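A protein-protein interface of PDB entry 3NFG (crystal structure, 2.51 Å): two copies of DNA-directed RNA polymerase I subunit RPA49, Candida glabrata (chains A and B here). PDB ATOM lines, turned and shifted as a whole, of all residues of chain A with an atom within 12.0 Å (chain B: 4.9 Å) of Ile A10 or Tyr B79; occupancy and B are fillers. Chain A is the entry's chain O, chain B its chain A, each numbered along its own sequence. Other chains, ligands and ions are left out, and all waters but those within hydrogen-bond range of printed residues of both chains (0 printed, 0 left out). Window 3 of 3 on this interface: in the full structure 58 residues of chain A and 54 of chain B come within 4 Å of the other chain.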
ATOM      1  N   ARG A   8     -18.577 -18.488 -22.406  1.00  0.00           N
ATOM      2  CA  ARG A   8     -17.518 -18.377 -21.396  1.00  0.00           C
ATOM      3  C   ARG A   8     -17.229 -16.897 -20.980  1.00  0.00           C
ATOM      4  O   ARG A   8     -17.820 -15.963 -21.537  1.00  0.00           O
ATOM      5  CB  ARG A   8     -16.200 -18.921 -21.958  1.00  0.00           C
ATOM      6  N   SER A   9     -16.350 -16.713 -19.970  1.00  0.00           N
ATOM      7  CA  SER A   9     -15.844 -15.451 -19.384  1.00  0.00           C
ATOM      8  C   SER A   9     -14.555 -15.796 -18.636  1.00  0.00           C
ATOM      9  O   SER A   9     -14.599 -16.729 -17.819  1.00  0.00           O
ATOM     10  CB  SER A   9     -16.896 -14.930 -18.400  1.00  0.00           C
ATOM     11  OG  SER A   9     -16.485 -13.731 -17.767  1.00  0.00           O
ATOM     12  N   ILE A  10     -13.413 -15.104 -18.923  1.00  0.00           N
ATOM     13  CA  ILE A  10     -12.129 -15.395 -18.245  1.00  0.00           C
ATOM     14  C   ILE A  10     -12.135 -14.857 -16.814  1.00  0.00           C
ATOM     15  O   ILE A  10     -12.239 -13.650 -16.631  1.00  0.00           O
ATOM     16  CB  ILE A  10     -10.850 -14.934 -19.013  1.00  0.00           C
ATOM     17  CG1 ILE A  10     -10.964 -15.049 -20.564  1.00  0.00           C
ATOM     18  CG2 ILE A  10      -9.583 -15.602 -18.455  1.00  0.00           C
ATOM     19  CD1 ILE A  10     -11.172 -16.470 -21.198  1.00  0.00           C
ATOM     20  N   ALA A  11     -12.002 -15.747 -15.805  1.00  0.00           N
ATOM     21  CA  ALA A  11     -12.020 -15.356 -14.404  1.00  0.00           C
ATOM     22  C   ALA A  11     -10.652 -14.941 -13.933  1.00  0.00           C
ATOM     23  O   ALA A  11      -9.668 -15.630 -14.215  1.00  0.00           O
ATOM     24  CB  ALA A  11     -12.538 -16.497 -13.554  1.00  0.00           C
ATOM     25  N   ILE A  12     -10.584 -13.813 -13.204  1.00  0.00           N
ATOM     26  CA  ILE A  12      -9.322 -13.348 -12.636  1.00  0.00           C
ATOM     27  C   ILE A  12      -9.177 -14.007 -11.258  1.00  0.00           C
ATOM     28  O   ILE A  12      -9.847 -13.608 -10.299  1.00  0.00           O
ATOM     29  CB  ILE A  12      -9.155 -11.802 -12.621  1.00  0.00           C
ATOM     30  CG1 ILE A  12      -9.189 -11.225 -14.047  1.00  0.00           C
ATOM     31  CG2 ILE A  12      -7.876 -11.411 -11.917  1.00  0.00           C
ATOM     32  CD1 ILE A  12      -9.672  -9.778 -14.151  1.00  0.00           C
ATOM     33  N   ASP A  13      -8.330 -15.052 -11.194  1.00  0.00           N
ATOM     34  CA  ASP A  13      -8.055 -15.825  -9.984  1.00  0.00           C
ATOM     35  C   ASP A  13      -7.146 -15.047  -9.045  1.00  0.00           C
ATOM     36  O   ASP A  13      -7.362 -15.056  -7.836  1.00  0.00           O
ATOM     37  CB  ASP A  13      -7.423 -17.187 -10.350  1.00  0.00           C
ATOM     38  CG  ASP A  13      -7.494 -18.259  -9.270  1.00  0.00           C
ATOM     39  OD1 ASP A  13      -8.608 -18.502  -8.743  1.00  0.00           O
ATOM     40  OD2 ASP A  13      -6.457 -18.915  -9.010  1.00  0.00           O
ATOM     41  N   SER A  14      -6.127 -14.382  -9.608  1.00  0.00           N
ATOM     42  CA  SER A  14      -5.146 -13.590  -8.879  1.00  0.00           C
ATOM     43  C   SER A  14      -4.512 -12.527  -9.785  1.00  0.00           C
ATOM     44  O   SER A  14      -4.330 -12.737 -10.988  1.00  0.00           O
ATOM     45  CB  SER A  14      -4.053 -14.484  -8.292  1.00  0.00           C
ATOM     46  OG  SER A  14      -3.281 -15.111  -9.302  1.00  0.00           O
ATOM     47  N   TYR A  15      -4.193 -11.378  -9.189  1.00  0.00           N
ATOM     48  CA  TYR A  15      -3.524 -10.271  -9.850  1.00  0.00           C
ATOM     49  C   TYR A  15      -2.435  -9.791  -8.914  1.00  0.00           C
ATOM     50  O   TYR A  15      -2.715  -9.438  -7.762  1.00  0.00           O
ATOM     51  CB  TYR A  15      -4.504  -9.141 -10.217  1.00  0.00           C
ATOM     52  CG  TYR A  15      -3.821  -7.890 -10.732  1.00  0.00           C
ATOM     53  CD1 TYR A  15      -2.952  -7.940 -11.818  1.00  0.00           C
ATOM     54  CD2 TYR A  15      -4.042  -6.653 -10.129  1.00  0.00           C
ATOM     55  CE1 TYR A  15      -2.297  -6.795 -12.272  1.00  0.00           C
ATOM     56  CE2 TYR A  15      -3.419  -5.499 -10.592  1.00  0.00           C
ATOM     57  CZ  TYR A  15      -2.542  -5.570 -11.663  1.00  0.00           C
ATOM     58  OH  TYR A  15      -1.936  -4.420 -12.122  1.00  0.00           O
ATOM     59  N   GLY B  77       0.343 -13.617 -18.015  1.00  0.00           N
ATOM     60  CA  GLY B  77      -0.778 -14.417 -17.538  1.00  0.00           C
ATOM     61  C   GLY B  77      -0.632 -15.909 -17.739  1.00  0.00           C
ATOM     62  O   GLY B  77      -0.083 -16.354 -18.757  1.00  0.00           O
ATOM     63  N   LEU B  78      -1.118 -16.688 -16.747  1.00  0.00           N
ATOM     64  CA  LEU B  78      -1.158 -18.146 -16.791  1.00  0.00           C
ATOM     65  C   LEU B  78      -2.620 -18.499 -16.863  1.00  0.00           C
ATOM     66  O   LEU B  78      -3.360 -18.287 -15.903  1.00  0.00           O
ATOM     67  CB  LEU B  78      -0.485 -18.774 -15.565  1.00  0.00           C
ATOM     68  CG  LEU B  78       1.026 -18.635 -15.522  1.00  0.00           C
ATOM     69  CD1 LEU B  78       1.548 -18.940 -14.161  1.00  0.00           C
ATOM     70  CD2 LEU B  78       1.688 -19.533 -16.547  1.00  0.00           C
ATOM     71  N   TYR B  79      -3.055 -18.913 -18.047  1.00  0.00           N
ATOM     72  CA  TYR B  79      -4.444 -19.240 -18.352  1.00  0.00           C
ATOM     73  C   TYR B  79      -4.699 -20.738 -18.326  1.00  0.00           C
ATOM     74  O   TYR B  79      -3.897 -21.518 -18.836  1.00  0.00           O
ATOM     75  CB  TYR B  79      -4.818 -18.655 -19.730  1.00  0.00           C
ATOM     76  CG  TYR B  79      -6.202 -19.011 -20.233  1.00  0.00           C
ATOM     77  CD1 TYR B  79      -7.340 -18.495 -19.624  1.00  0.00           C
ATOM     78  CD2 TYR B  79      -6.370 -19.796 -21.371  1.00  0.00           C
ATOM     79  CE1 TYR B  79      -8.613 -18.785 -20.107  1.00  0.00           C
ATOM     80  CE2 TYR B  79      -7.637 -20.068 -21.882  1.00  0.00           C
ATOM     81  CZ  TYR B  79      -8.758 -19.564 -21.244  1.00  0.00           C
ATOM     82  OH  TYR B  79     -10.017 -19.833 -21.725  1.00  0.00           O
ATOM     83  N   ASP B  80      -5.835 -21.122 -17.748  1.00  0.00           N
ATOM     84  CA  ASP B  80      -6.278 -22.509 -17.665  1.00  0.00           C
ATOM     85  C   ASP B  80      -7.450 -22.728 -18.642  1.00  0.00           C
ATOM     86  O   ASP B  80      -8.574 -22.298 -18.358  1.00  0.00           O
ATOM     87  CB  ASP B  80      -6.689 -22.854 -16.220  1.00  0.00           C
ATOM     88  CG  ASP B  80      -6.764 -24.333 -15.924  1.00  0.00           C
ATOM     89  OD1 ASP B  80      -7.582 -25.025 -16.566  1.00  0.00           O
ATOM     90  OD2 ASP B  80      -6.028 -24.793 -15.034  1.00  0.00           O
ATOM     91  N   LYS B  81      -7.168 -23.379 -19.802  1.00  0.00           N
ATOM     92  CA  LYS B  81      -8.129 -23.705 -20.872  1.00  0.00           C
ATOM     93  C   LYS B  81      -9.413 -24.328 -20.293  1.00  0.00           C
ATOM     94  O   LYS B  81     -10.523 -23.902 -20.637  1.00  0.00           O
ATOM     95  CB  LYS B  81      -7.510 -24.700 -21.883  1.00  0.00           C
ATOM     96  CG  LYS B  81      -6.308 -24.203 -22.693  1.00  0.00           C
ATOM     97  CD  LYS B  81      -5.585 -25.380 -23.343  1.00  0.00           C
ATOM     98  CE  LYS B  81      -4.568 -24.961 -24.370  1.00  0.00           C
ATOM     99  NZ  LYS B  81      -3.807 -26.121 -24.894  1.00  0.00           N
ATOM    100  N   GLY B  84     -11.074 -21.922 -17.190  1.00  0.00           N
ATOM    101  CA  GLY B  84     -11.366 -20.581 -17.694  1.00  0.00           C
ATOM    102  C   GLY B  84     -10.928 -19.515 -16.709  1.00  0.00           C
ATOM    103  O   GLY B  84     -11.601 -18.494 -16.544  1.00  0.00           O
ATOM    104  N   LYS B  85      -9.803 -19.774 -16.029  1.00  0.00           N
ATOM    105  CA  LYS B  85      -9.239 -18.905 -15.008  1.00  0.00           C
ATOM    106  C   LYS B  85      -7.844 -18.455 -15.419  1.00  0.00           C
ATOM    107  O   LYS B  85      -7.087 -19.221 -16.027  1.00  0.00           O
ATOM    108  CB  LYS B  85      -9.188 -19.633 -13.648  1.00  0.00           C
ATOM    109  CG  LYS B  85     -10.560 -19.925 -13.036  1.00  0.00           C
ATOM    110  CD  LYS B  85     -10.443 -20.505 -11.627  1.00  0.00           C
ATOM    111  CE  LYS B  85     -11.773 -20.510 -10.902  1.00  0.00           C
ATOM    112  NZ  LYS B  85     -11.692 -21.151  -9.567  1.00  0.00           N
ATOM    113  N   ILE B  86      -7.511 -17.211 -15.073  1.00  0.00           N
ATOM    114  CA  ILE B  86      -6.210 -16.611 -15.344  1.00  0.00           C
ATOM    115  C   ILE B  86      -5.548 -16.109 -14.050  1.00  0.00           C
ATOM    116  O   ILE B  86      -6.234 -15.667 -13.125  1.00  0.00           O
ATOM    117  CB  ILE B  86      -6.296 -15.514 -16.459  1.00  0.00           C
ATOM    118  CG1 ILE B  86      -4.906 -15.188 -17.040  1.00  0.00           C
ATOM    119  CG2 ILE B  86      -7.038 -14.243 -15.990  1.00  0.00           C
ATOM    120  CD1 ILE B  86      -4.877 -14.878 -18.469  1.00  0.00           C
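N of Asp A13 lies within hydrogen-bond range of O of Ile B86. N of Ile B86 sits at hydrogen-bond distance from O of Ala A11, at 2.8 Å. The backbone NH of Ala A11 lies within hydrogen-bond range of the backbone carbonyl oxygen of Gly B84, at 2.9 Å.
The backbone NH of Asp B80 is in hydrogen-bond range of the backbone carbonyl oxygen of Lys B85 (2.9 Å).
Among the printed residues, pairs that only touch across the chains: Ser A9 with Gly B84 (3.7 Å), Ile A10 with Tyr B79 (3.6 Å), Ile A10 with Gly B84 (3.6 Å), Ile A10 with Ile B86 (3.8 Å), Ala A11 with Lys B85 (3.4 Å), Ile A12 with Ile B86 (3.9 Å), Asp A13 with Lys B85 (3.96 Å) and Ser A14 with Ile B86 (3.7 Å).
Arg A8 touches none of the printed residues of chain B. Of the printed residues of chain B, Ser A9 touches Gly B84. Ile A10 touches three residues of chain B. Printed residues of chain B within 4 Å of Ala A11: Gly B84, Lys B85 and Ile B86. Printed residues of chain B within 4 Å of Ile A12: Ile B86. Tyr A15 touches none of the printed residues of chain B. No residue of chain A comes within 4 Å of Gly B77. Tyr B79 touches just one residue of chain A: Ile A10. Of chain A, only Ser A9 (3.7 Å), Ile A10 (3.6 Å) and Ala A11 (2.9 Å) come within 4 Å of Gly B84. The nearest printed residue of chain B that does not touch Ile A12 is Lys B85 (5.6 Å).
Of the 8 printed residues of chain A, 6 touch a printed residue of chain B. Printed residues of chain A that touch a printed residue of chain B: Ser A9, Ile A10, Ala A11, Ile A12, Asp A13 and Ser A14. Of the 8 printed residues of chain B, 4 touch a printed residue of chain A. Along chain B the printed residues that touch a printed residue of chain A span positions 79 to 86. Among the printed residues, 11 pairs touch across the chains. Among the printed residues, no Asp or Glu carboxylate lies within 4 Å of a Lys or Arg side-chain nitrogen of the other chain.
No position is printed for both chains. Of the 11 pairs that touch across the chains among the printed residues, none has its exchanged pair printed and touching as well.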
